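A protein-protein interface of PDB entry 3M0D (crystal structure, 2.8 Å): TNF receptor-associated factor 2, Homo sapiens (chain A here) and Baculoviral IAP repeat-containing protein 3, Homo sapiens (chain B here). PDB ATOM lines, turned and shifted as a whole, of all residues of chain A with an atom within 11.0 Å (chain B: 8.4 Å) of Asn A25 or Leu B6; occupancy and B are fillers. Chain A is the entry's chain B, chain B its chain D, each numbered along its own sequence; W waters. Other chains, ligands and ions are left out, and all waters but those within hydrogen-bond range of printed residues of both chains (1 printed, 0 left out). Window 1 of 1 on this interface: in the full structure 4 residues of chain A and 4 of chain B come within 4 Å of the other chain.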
ATOM      1  N   PHE A  17       1.089  16.934  10.992  1.00  0.00           N
ATOM      2  CA  PHE A  17       1.963  16.076  10.210  1.00  0.00           C
ATOM      3  C   PHE A  17       1.838  16.328   8.728  1.00  0.00           C
ATOM      4  O   PHE A  17       2.817  16.175   8.001  1.00  0.00           O
ATOM      5  CB  PHE A  17       1.730  14.597  10.522  1.00  0.00           C
ATOM      6  CG  PHE A  17       2.446  14.132  11.743  1.00  0.00           C
ATOM      7  CD1 PHE A  17       3.331  14.982  12.396  1.00  0.00           C
ATOM      8  CD2 PHE A  17       2.243  12.860  12.245  1.00  0.00           C
ATOM      9  CE1 PHE A  17       3.996  14.575  13.536  1.00  0.00           C
ATOM     10  CE2 PHE A  17       2.910  12.440  13.396  1.00  0.00           C
ATOM     11  CZ  PHE A  17       3.784  13.297  14.042  1.00  0.00           C
ATOM     12  N   GLU A  18       0.646  16.720   8.284  1.00  0.00           N
ATOM     13  CA  GLU A  18       0.425  17.023   6.871  1.00  0.00           C
ATOM     14  C   GLU A  18       1.321  18.145   6.366  1.00  0.00           C
ATOM     15  O   GLU A  18       1.977  18.012   5.308  1.00  0.00           O
ATOM     16  CB  GLU A  18      -1.012  17.411   6.601  1.00  0.00           C
ATOM     17  CG  GLU A  18      -1.866  16.301   6.035  1.00  0.00           C
ATOM     18  CD  GLU A  18      -3.299  16.742   5.817  1.00  0.00           C
ATOM     19  OE1 GLU A  18      -3.489  17.744   5.081  1.00  0.00           O
ATOM     20  OE2 GLU A  18      -4.221  16.104   6.394  1.00  0.00           O
ATOM     21  N   ASN A  19       1.346  19.253   7.109  1.00  0.00           N
ATOM     22  CA  ASN A  19       2.143  20.386   6.667  1.00  0.00           C
ATOM     23  C   ASN A  19       3.645  20.144   6.775  1.00  0.00           C
ATOM     24  O   ASN A  19       4.427  20.644   5.945  1.00  0.00           O
ATOM     25  CB  ASN A  19       1.745  21.691   7.348  1.00  0.00           C
ATOM     26  CG  ASN A  19       2.046  22.887   6.475  1.00  0.00           C
ATOM     27  OD1 ASN A  19       3.058  23.568   6.651  1.00  0.00           O
ATOM     28  ND2 ASN A  19       1.191  23.115   5.483  1.00  0.00           N
ATOM     29  N   ILE A  20       4.039  19.362   7.779  1.00  0.00           N
ATOM     30  CA  ILE A  20       5.416  18.897   7.883  1.00  0.00           C
ATOM     31  C   ILE A  20       5.863  18.186   6.604  1.00  0.00           C
ATOM     32  O   ILE A  20       6.866  18.582   5.984  1.00  0.00           O
ATOM     33  CB  ILE A  20       5.609  17.980   9.092  1.00  0.00           C
ATOM     34  CG1 ILE A  20       5.702  18.818  10.369  1.00  0.00           C
ATOM     35  CG2 ILE A  20       6.837  17.108   8.911  1.00  0.00           C
ATOM     36  CD1 ILE A  20       5.875  17.991  11.650  1.00  0.00           C
ATOM     37  N   VAL A  21       5.119  17.151   6.213  1.00  0.00           N
ATOM     38  CA  VAL A  21       5.407  16.411   4.987  1.00  0.00           C
ATOM     39  C   VAL A  21       5.405  17.325   3.780  1.00  0.00           C
ATOM     40  O   VAL A  21       6.262  17.209   2.903  1.00  0.00           O
ATOM     41  CB  VAL A  21       4.356  15.332   4.734  1.00  0.00           C
ATOM     42  CG1 VAL A  21       4.540  14.707   3.362  1.00  0.00           C
ATOM     43  CG2 VAL A  21       4.420  14.281   5.808  1.00  0.00           C
ATOM     44  N   CYS A  22       4.432  18.232   3.735  1.00  0.00           N
ATOM     45  CA  CYS A  22       4.256  19.119   2.595  1.00  0.00           C
ATOM     46  C   CYS A  22       5.469  20.038   2.427  1.00  0.00           C
ATOM     47  O   CYS A  22       5.957  20.268   1.317  1.00  0.00           O
ATOM     48  CB  CYS A  22       2.961  19.919   2.752  1.00  0.00           C
ATOM     49  SG  CYS A  22       2.468  20.836   1.263  1.00  0.00           S
ATOM     50  N   VAL A  23       5.965  20.542   3.546  1.00  0.00           N
ATOM     51  CA  VAL A  23       7.193  21.310   3.551  1.00  0.00           C
ATOM     52  C   VAL A  23       8.437  20.493   3.162  1.00  0.00           C
ATOM     53  O   VAL A  23       9.209  20.912   2.295  1.00  0.00           O
ATOM     54  CB  VAL A  23       7.417  21.941   4.914  1.00  0.00           C
ATOM     55  CG1 VAL A  23       8.834  22.463   5.009  1.00  0.00           C
ATOM     56  CG2 VAL A  23       6.414  23.049   5.145  1.00  0.00           C
ATOM     57  N   LEU A  24       8.635  19.348   3.813  1.00  0.00           N
ATOM     58  CA  LEU A  24       9.764  18.463   3.518  1.00  0.00           C
ATOM     59  C   LEU A  24       9.816  18.127   2.050  1.00  0.00           C
ATOM     60  O   LEU A  24      10.888  18.088   1.439  1.00  0.00           O
ATOM     61  CB  LEU A  24       9.630  17.150   4.283  1.00  0.00           C
ATOM     62  CG  LEU A  24      10.292  17.093   5.649  1.00  0.00           C
ATOM     63  CD1 LEU A  24       9.733  15.927   6.427  1.00  0.00           C
ATOM     64  CD2 LEU A  24      11.816  17.005   5.519  1.00  0.00           C
ATOM     65  N   ASN A  25       8.647  17.853   1.483  1.00  0.00           N
ATOM     66  CA  ASN A  25       8.579  17.544   0.075  1.00  0.00           C
ATOM     67  C   ASN A  25       9.148  18.681  -0.794  1.00  0.00           C
ATOM     68  O   ASN A  25       9.895  18.434  -1.747  1.00  0.00           O
ATOM     69  CB  ASN A  25       7.156  17.217  -0.315  1.00  0.00           C
ATOM     70  CG  ASN A  25       7.046  16.811  -1.754  1.00  0.00           C
ATOM     71  OD1 ASN A  25       7.863  16.054  -2.243  1.00  0.00           O
ATOM     72  ND2 ASN A  25       6.054  17.340  -2.454  1.00  0.00           N
ATOM     73  N   ARG A  26       8.806  19.923  -0.456  1.00  0.00           N
ATOM     74  CA  ARG A  26       9.418  21.065  -1.111  1.00  0.00           C
ATOM     75  C   ARG A  26      10.926  21.109  -0.869  1.00  0.00           C
ATOM     76  O   ARG A  26      11.719  21.197  -1.814  1.00  0.00           O
ATOM     77  CB  ARG A  26       8.785  22.360  -0.630  1.00  0.00           C
ATOM     78  CG  ARG A  26       7.501  22.688  -1.329  1.00  0.00           C
ATOM     79  CD  ARG A  26       6.996  24.053  -0.924  1.00  0.00           C
ATOM     80  NE  ARG A  26       5.542  24.100  -1.036  1.00  0.00           N
ATOM     81  CZ  ARG A  26       4.708  24.093   0.001  1.00  0.00           C
ATOM     82  NH1 ARG A  26       5.177  24.068   1.244  1.00  0.00           N
ATOM     83  NH2 ARG A  26       3.399  24.128  -0.209  1.00  0.00           N
ATOM     84  N   GLU A  27      11.322  21.049   0.397  1.00  0.00           N
ATOM     85  CA  GLU A  27      12.735  21.155   0.733  1.00  0.00           C
ATOM     86  C   GLU A  27      13.602  20.065   0.089  1.00  0.00           C
ATOM     87  O   GLU A  27      14.692  20.347  -0.402  1.00  0.00           O
ATOM     88  CB  GLU A  27      12.909  21.213   2.242  1.00  0.00           C
ATOM     89  CG  GLU A  27      12.088  22.338   2.852  1.00  0.00           C
ATOM     90  CD  GLU A  27      12.156  22.372   4.368  1.00  0.00           C
ATOM     91  OE1 GLU A  27      12.744  21.439   4.961  1.00  0.00           O
ATOM     92  OE2 GLU A  27      11.619  23.334   4.964  1.00  0.00           O
ATOM     93  N   VAL A  28      13.109  18.831   0.057  1.00  0.00           N
ATOM     94  CA  VAL A  28      13.849  17.736  -0.572  1.00  0.00           C
ATOM     95  C   VAL A  28      13.945  17.910  -2.089  1.00  0.00           C
ATOM     96  O   VAL A  28      15.013  17.730  -2.670  1.00  0.00           O
ATOM     97  CB  VAL A  28      13.233  16.355  -0.231  1.00  0.00           C
ATOM     98  CG1 VAL A  28      13.901  15.258  -1.030  1.00  0.00           C
ATOM     99  CG2 VAL A  28      13.359  16.073   1.249  1.00  0.00           C
ATOM    100  N   GLU A  29      12.835  18.256  -2.730  1.00  0.00           N
ATOM    101  CA  GLU A  29      12.865  18.606  -4.150  1.00  0.00           C
ATOM    102  C   GLU A  29      13.900  19.720  -4.444  1.00  0.00           C
ATOM    103  O   GLU A  29      14.701  19.621  -5.381  1.00  0.00           O
ATOM    104  CB  GLU A  29      11.480  19.068  -4.590  1.00  0.00           C
ATOM    105  CG  GLU A  29      11.203  18.992  -6.088  1.00  0.00           C
ATOM    106  CD  GLU A  29       9.785  19.439  -6.472  1.00  0.00           C
ATOM    107  OE1 GLU A  29       9.425  19.293  -7.665  1.00  0.00           O
ATOM    108  OE2 GLU A  29       9.032  19.932  -5.595  1.00  0.00           O
ATOM    109  N   ARG A  30      13.870  20.774  -3.631  1.00  0.00           N
ATOM    110  CA  ARG A  30      14.738  21.924  -3.810  1.00  0.00           C
ATOM    111  C   ARG A  30      16.200  21.519  -3.669  1.00  0.00           C
ATOM    112  O   ARG A  30      17.040  21.897  -4.474  1.00  0.00           O
ATOM    113  CB  ARG A  30      14.402  23.011  -2.786  1.00  0.00           C
ATOM    114  CG  ARG A  30      14.846  24.413  -3.192  1.00  0.00           C
ATOM    115  CD  ARG A  30      14.917  25.395  -2.011  1.00  0.00           C
ATOM    116  NE  ARG A  30      14.257  24.888  -0.802  1.00  0.00           N
ATOM    117  CZ  ARG A  30      13.078  25.303  -0.332  1.00  0.00           C
ATOM    118  NH1 ARG A  30      12.394  26.252  -0.962  1.00  0.00           N
ATOM    119  NH2 ARG A  30      12.588  24.763   0.780  1.00  0.00           N
ATOM    120  N   VAL A  31      16.501  20.752  -2.632  1.00  0.00           N
ATOM    121  CA  VAL A  31      17.865  20.305  -2.392  1.00  0.00           C
ATOM    122  C   VAL A  31      18.371  19.387  -3.502  1.00  0.00           C
ATOM    123  O   VAL A  31      19.486  19.570  -3.985  1.00  0.00           O
ATOM    124  CB  VAL A  31      17.990  19.615  -1.020  1.00  0.00           C
ATOM    125  CG1 VAL A  31      19.164  18.717  -1.008  1.00  0.00           C
ATOM    126  CG2 VAL A  31      18.132  20.652   0.080  1.00  0.00           C
ATOM    127  N   ALA A  32      17.551  18.411  -3.900  1.00  0.00           N
ATOM    128  CA  ALA A  32      17.858  17.549  -5.041  1.00  0.00           C
ATOM    129  C   ALA A  32      18.264  18.385  -6.262  1.00  0.00           C
ATOM    130  O   ALA A  32      19.253  18.096  -6.949  1.00  0.00           O
ATOM    131  CB  ALA A  32      16.666  16.700  -5.383  1.00  0.00           C
ATOM    132  N   MET A  33      17.435  19.393  -6.524  1.00  0.00           N
ATOM    133  CA  MET A  33      17.622  20.407  -7.542  1.00  0.00           C
ATOM    134  C   MET A  33      19.023  21.012  -7.494  1.00  0.00           C
ATOM    135  O   MET A  33      19.731  21.072  -8.501  1.00  0.00           O
ATOM    136  CB  MET A  33      16.617  21.526  -7.259  1.00  0.00           C
ATOM    137  CG  MET A  33      16.020  22.225  -8.463  1.00  0.00           C
ATOM    138  SD  MET A  33      14.795  21.204  -9.286  1.00  0.00           S
ATOM    139  CE  MET A  33      15.842  19.989 -10.120  1.00  0.00           C
ATOM    140  N   THR A  34      19.386  21.490  -6.311  1.00  0.00           N
ATOM    141  CA  THR A  34      20.645  22.157  -6.064  1.00  0.00           C
ATOM    142  C   THR A  34      21.798  21.242  -6.366  1.00  0.00           C
ATOM    143  O   THR A  34      22.719  21.607  -7.110  1.00  0.00           O
ATOM    144  CB  THR A  34      20.764  22.538  -4.591  1.00  0.00           C
ATOM    145  OG1 THR A  34      19.883  23.632  -4.305  1.00  0.00           O
ATOM    146  CG2 THR A  34      22.185  22.952  -4.275  1.00  0.00           C
ATOM    147  N   MET B   1      -5.811  17.973   3.308  1.00  0.00           N
ATOM    148  CA  MET B   1      -5.374  16.704   2.732  1.00  0.00           C
ATOM    149  C   MET B   1      -4.204  16.897   1.762  1.00  0.00           C
ATOM    150  O   MET B   1      -3.977  18.000   1.245  1.00  0.00           O
ATOM    151  CB  MET B   1      -6.538  15.991   2.046  1.00  0.00           C
ATOM    152  CG  MET B   1      -6.254  14.535   1.708  1.00  0.00           C
ATOM    153  SD  MET B   1      -7.736  13.528   1.475  1.00  0.00           S
ATOM    154  CE  MET B   1      -8.536  13.675   3.074  1.00  0.00           C
ATOM    155  N   LEU B   2      -3.458  15.818   1.530  1.00  0.00           N
ATOM    156  CA  LEU B   2      -2.259  15.853   0.689  1.00  0.00           C
ATOM    157  C   LEU B   2      -2.623  15.622  -0.773  1.00  0.00           C
ATOM    158  O   LEU B   2      -3.666  15.036  -1.072  1.00  0.00           O
ATOM    159  CB  LEU B   2      -1.257  14.797   1.169  1.00  0.00           C
ATOM    160  CG  LEU B   2       0.095  15.283   1.697  1.00  0.00           C
ATOM    161  CD1 LEU B   2      -0.030  16.422   2.677  1.00  0.00           C
ATOM    162  CD2 LEU B   2       0.859  14.129   2.315  1.00  0.00           C
ATOM    163  N   SER B   3      -1.763  16.058  -1.685  1.00  0.00           N
ATOM    164  CA  SER B   3      -2.097  15.979  -3.099  1.00  0.00           C
ATOM    165  C   SER B   3      -2.155  14.540  -3.597  1.00  0.00           C
ATOM    166  O   SER B   3      -1.503  13.654  -3.064  1.00  0.00           O
ATOM    167  CB  SER B   3      -1.111  16.793  -3.933  1.00  0.00           C
ATOM    168  OG  SER B   3       0.159  16.185  -3.950  1.00  0.00           O
ATOM    169  N   CYS B   4      -2.951  14.310  -4.627  1.00  0.00           N
ATOM    170  CA  CYS B   4      -2.995  13.005  -5.255  1.00  0.00           C
ATOM    171  C   CYS B   4      -1.622  12.565  -5.734  1.00  0.00           C
ATOM    172  O   CYS B   4      -1.318  11.378  -5.679  1.00  0.00           O
ATOM    173  CB  CYS B   4      -3.984  13.008  -6.417  1.00  0.00           C
ATOM    174  SG  CYS B   4      -5.687  12.953  -5.870  1.00  0.00           S
ATOM    175  N   GLU B   5      -0.801  13.509  -6.211  1.00  0.00           N
ATOM    176  CA  GLU B   5       0.606  13.214  -6.539  1.00  0.00           C
ATOM    177  C   GLU B   5       1.402  12.618  -5.359  1.00  0.00           C
ATOM    178  O   GLU B   5       2.086  11.600  -5.507  1.00  0.00           O
ATOM    179  CB  GLU B   5       1.304  14.470  -7.028  1.00  0.00           C
ATOM    180  CG  GLU B   5       2.735  14.269  -7.462  1.00  0.00           C
ATOM    181  CD  GLU B   5       3.255  15.483  -8.226  1.00  0.00           C
ATOM    182  OE1 GLU B   5       4.496  15.594  -8.432  1.00  0.00           O
ATOM    183  OE2 GLU B   5       2.406  16.323  -8.626  1.00  0.00           O
ATOM    184  N   LEU B   6       1.311  13.254  -4.192  1.00  0.00           N
ATOM    185  CA  LEU B   6       1.960  12.732  -2.989  1.00  0.00           C
ATOM    186  C   LEU B   6       1.466  11.336  -2.576  1.00  0.00           C
ATOM    187  O   LEU B   6       2.255  10.448  -2.271  1.00  0.00           O
ATOM    188  CB  LEU B   6       1.816  13.720  -1.834  1.00  0.00           C
ATOM    189  CG  LEU B   6       2.908  14.788  -1.902  1.00  0.00           C
ATOM    190  CD1 LEU B   6       2.692  15.912  -0.916  1.00  0.00           C
ATOM    191  CD2 LEU B   6       4.236  14.144  -1.649  1.00  0.00           C
ATOM    192  N   TYR B   7       0.157  11.148  -2.574  1.00  0.00           N
ATOM    193  CA  TYR B   7      -0.409   9.848  -2.294  1.00  0.00           C
ATOM    194  C   TYR B   7       0.081   8.795  -3.284  1.00  0.00           C
ATOM    195  O   TYR B   7       0.293   7.636  -2.911  1.00  0.00           O
ATOM    196  CB  TYR B   7      -1.933   9.940  -2.307  1.00  0.00           C
ATOM    197  CG  TYR B   7      -2.527  10.354  -0.987  1.00  0.00           C
ATOM    198  CD1 TYR B   7      -2.379  11.652  -0.515  1.00  0.00           C
ATOM    199  CD2 TYR B   7      -3.250   9.439  -0.207  1.00  0.00           C
ATOM    200  CE1 TYR B   7      -2.937  12.034   0.710  1.00  0.00           C
ATOM    201  CE2 TYR B   7      -3.811   9.805   1.018  1.00  0.00           C
ATOM    202  CZ  TYR B   7      -3.652  11.103   1.469  1.00  0.00           C
ATOM    203  OH  TYR B   7      -4.195  11.468   2.678  1.00  0.00           O
ATOM    204  N   ARG B   8       0.243   9.194  -4.542  1.00  0.00           N
ATOM    205  CA  ARG B   8       0.865   8.328  -5.548  1.00  0.00           C
ATOM    206  C   ARG B   8       2.334   8.067  -5.222  1.00  0.00           C
ATOM    207  O   ARG B   8       2.819   6.951  -5.387  1.00  0.00           O
ATOM    208  CB  ARG B   8       0.746   8.925  -6.956  1.00  0.00           C
ATOM    209  CG  ARG B   8      -0.492   8.475  -7.721  1.00  0.00           C
ATOM    210  CD  ARG B   8      -0.341   8.773  -9.210  1.00  0.00           C
ATOM    211  NE  ARG B   8       0.004  10.176  -9.483  1.00  0.00           N
ATOM    212  CZ  ARG B   8      -0.863  11.198  -9.459  1.00  0.00           C
ATOM    213  NH1 ARG B   8      -2.156  11.005  -9.154  1.00  0.00           N
ATOM    214  NH2 ARG B   8      -0.435  12.431  -9.718  1.00  0.00           N
ATOM    215  N   MET B   9       3.043   9.095  -4.762  1.00  0.00           N
ATOM    216  CA  MET B   9       4.444   8.935  -4.415  1.00  0.00           C
ATOM    217  C   MET B   9       4.616   7.937  -3.281  1.00  0.00           C
ATOM    218  O   MET B   9       5.487   7.079  -3.334  1.00  0.00           O
ATOM    219  CB  MET B   9       5.022  10.262  -3.986  1.00  0.00           C
ATOM    220  CG  MET B   9       6.496  10.408  -4.271  1.00  0.00           C
ATOM    221  SD  MET B   9       7.161  11.829  -3.368  1.00  0.00           S
ATOM    222  CE  MET B   9       8.763  11.923  -4.144  1.00  0.00           C
ATOM    223  N   SER B  10       3.790   8.062  -2.248  1.00  0.00           N
ATOM    224  CA  SER B  10       3.875   7.199  -1.072  1.00  0.00           C
ATOM    225  C   SER B  10       3.851   5.703  -1.424  1.00  0.00           C
ATOM    226  O   SER B  10       4.159   4.853  -0.569  1.00  0.00           O
ATOM    227  CB  SER B  10       2.766   7.531  -0.068  1.00  0.00           C
ATOM    228  OG  SER B  10       1.525   6.962  -0.460  1.00  0.00           O
ATOM    229  N   THR B  11       3.508   5.382  -2.674  1.00  0.00           N
ATOM    230  CA  THR B  11       3.472   3.976  -3.101  1.00  0.00           C
ATOM    231  C   THR B  11       4.847   3.452  -3.516  1.00  0.00           C
ATOM    232  O   THR B  11       4.986   2.325  -4.021  1.00  0.00           O
ATOM    233  CB  THR B  11       2.441   3.707  -4.235  1.00  0.00           C
ATOM    234  OG1 THR B  11       2.844   4.351  -5.454  1.00  0.00           O
ATOM    235  CG2 THR B  11       1.039   4.183  -3.819  1.00  0.00           C
ATOM    236  N   TYR B  12       5.867   4.273  -3.296  1.00  0.00           N
ATOM    237  CA  TYR B  12       7.192   3.980  -3.830  1.00  0.00           C
ATOM    238  C   TYR B  12       8.248   3.649  -2.745  1.00  0.00           C
ATOM    239  O   TYR B  12       9.452   3.659  -3.005  1.00  0.00           O
ATOM    240  CB  TYR B  12       7.654   5.142  -4.736  1.00  0.00           C
ATOM    241  CG  TYR B  12       6.961   5.227  -6.087  1.00  0.00           C
ATOM    242  CD1 TYR B  12       7.485   4.572  -7.205  1.00  0.00           C
ATOM    243  CD2 TYR B  12       5.801   5.993  -6.257  1.00  0.00           C
ATOM    244  CE1 TYR B  12       6.864   4.658  -8.453  1.00  0.00           C
ATOM    245  CE2 TYR B  12       5.167   6.079  -7.488  1.00  0.00           C
ATOM    246  CZ  TYR B  12       5.699   5.410  -8.585  1.00  0.00           C
ATOM    247  OH  TYR B  12       5.077   5.497  -9.812  1.00  0.00           O
ATOM    248  N   GLU B  23      11.405   8.350  -8.307  1.00  0.00           N
ATOM    249  CA  GLU B  23      10.022   8.035  -7.989  1.00  0.00           C
ATOM    250  C   GLU B  23       9.203   9.294  -8.051  1.00  0.00           C
ATOM    251  O   GLU B  23       7.985   9.228  -8.167  1.00  0.00           O
ATOM    252  CB  GLU B  23       9.898   7.391  -6.618  1.00  0.00           C
ATOM    253  CG  GLU B  23      10.717   6.126  -6.472  1.00  0.00           C
ATOM    254  CD  GLU B  23      12.085   6.393  -5.882  1.00  0.00           C
ATOM    255  OE1 GLU B  23      12.541   7.558  -5.933  1.00  0.00           O
ATOM    256  OE2 GLU B  23      12.695   5.437  -5.353  1.00  0.00           O
ATOM    257  N   ARG B  24       9.884  10.441  -8.010  1.00  0.00           N
ATOM    258  CA  ARG B  24       9.192  11.726  -8.040  1.00  0.00           C
ATOM    259  C   ARG B  24       8.537  12.026  -9.375  1.00  0.00           C
ATOM    260  O   ARG B  24       7.355  12.332  -9.429  1.00  0.00           O
ATOM    261  CB  ARG B  24      10.088  12.886  -7.623  1.00  0.00           C
ATOM    262  CG  ARG B  24       9.322  14.215  -7.625  1.00  0.00           C
ATOM    263  CD  ARG B  24      10.147  15.415  -7.178  1.00  0.00           C
ATOM    264  NE  ARG B  24      10.558  15.308  -5.788  1.00  0.00           N
ATOM    265  CZ  ARG B  24       9.816  15.700  -4.760  1.00  0.00           C
ATOM    266  NH1 ARG B  24       8.628  16.249  -4.980  1.00  0.00           N
ATOM    267  NH2 ARG B  24      10.266  15.560  -3.518  1.00  0.00           N
ATOM    268  N   ALA B  27       5.684   9.531 -10.187  1.00  0.00           N
ATOM    269  CA  ALA B  27       4.437   9.933  -9.572  1.00  0.00           C
ATOM    270  C   ALA B  27       3.807  11.193 -10.254  1.00  0.00           C
ATOM    271  O   ALA B  27       2.611  11.226 -10.545  1.00  0.00           O
ATOM    272  CB  ALA B  27       4.659  10.138  -8.079  1.00  0.00           C
ATOM    273  N   ARG B  28       4.618  12.210 -10.529  1.00  0.00           N
ATOM    274  CA  ARG B  28       4.150  13.414 -11.219  1.00  0.00           C
ATOM    275  C   ARG B  28       3.573  13.106 -12.596  1.00  0.00           C
ATOM    276  O   ARG B  28       2.704  13.832 -13.097  1.00  0.00           O
ATOM    277  CB  ARG B  28       5.295  14.419 -11.359  1.00  0.00           C
ATOM    278  CG  ARG B  28       4.886  15.739 -11.990  1.00  0.00           C
ATOM    279  CD  ARG B  28       6.034  16.706 -11.986  1.00  0.00           C
ATOM    280  NE  ARG B  28       7.249  16.087 -12.508  1.00  0.00           N
ATOM    281  CZ  ARG B  28       8.445  16.202 -11.932  1.00  0.00           C
ATOM    282  NH1 ARG B  28       8.558  16.912 -10.811  1.00  0.00           N
ATOM    283  NH2 ARG B  28       9.519  15.611 -12.470  1.00  0.00           N
HETATM  284  O   HOH W   1       6.739  17.863  -8.294  1.00  0.00           O
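The backbone NH (N) of Met B1 is in hydrogen-bond range of the side-chain carboxylate (OE1) of Glu A18 (2.9 Å).
The side-chain amide oxygen (OD1) of Asn A25 sits at hydrogen-bond distance from the guanidinium group (NH2) of Arg B24 (2.8 Å).
OE2 of Glu A29 is in salt-bridge range of NH1 of Arg B24 (3.8 Å).
The side-chain hydroxyl (OG) of Ser B3 sits at hydrogen-bond distance from the backbone NH (N) of Leu B6 (3.2 Å).
O of Glu A18 touches CD1 of Leu B2 (3.7 Å).
Val A21 touches Leu B2 (CG1 to CD2, 3.9 Å).
Asn A25 touches Leu B6 (ND2 to CD2, 3.8 Å).
Printed residues of chain B within 4 Å of Asn A25: Leu B6 and Arg B24.
Leu B2 touches just these residues of chain A: Glu A18 (3.7 Å) and Val A21 (3.9 Å).
No residue of chain A comes within 4 Å of Ser B3.
No residue of chain A comes within 4 Å of Glu B5.
Arg B8 touches none of the printed residues of chain A.
No residue of chain A comes within 4 Å of Ser B10.
Of the printed residues of chain B, Glu A29 touches Arg B24.
Printed residues of chain A within 4 Å of Arg B24: Asn A25 and Glu A29.
Arg B28 touches none of the printed residues of chain A.
Arg A30 touches none of the printed residues of chain B.
The nearest residue of chain A that does not touch Leu B6 is Val A21 (4.8 Å).
Of the 18 printed residues of chain A, 4 touch a printed residue of chain B.
Hydrophobic or aromatic side chains of chain A that line the printed part of chain B: Val A21.
Along chain A the printed residues that touch a printed residue of chain B span positions 18 to 29.
Of the 16 printed residues of chain B, 4 touch a printed residue of chain A.
Hydrophobic or aromatic side chains of chain B that line the printed part of chain A: Leu B2 and Leu B6.
Water W1 lies within hydrogen-bond range of OE1 of Glu A29, OE1 of Glu B5 and NH1 of Arg B28.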
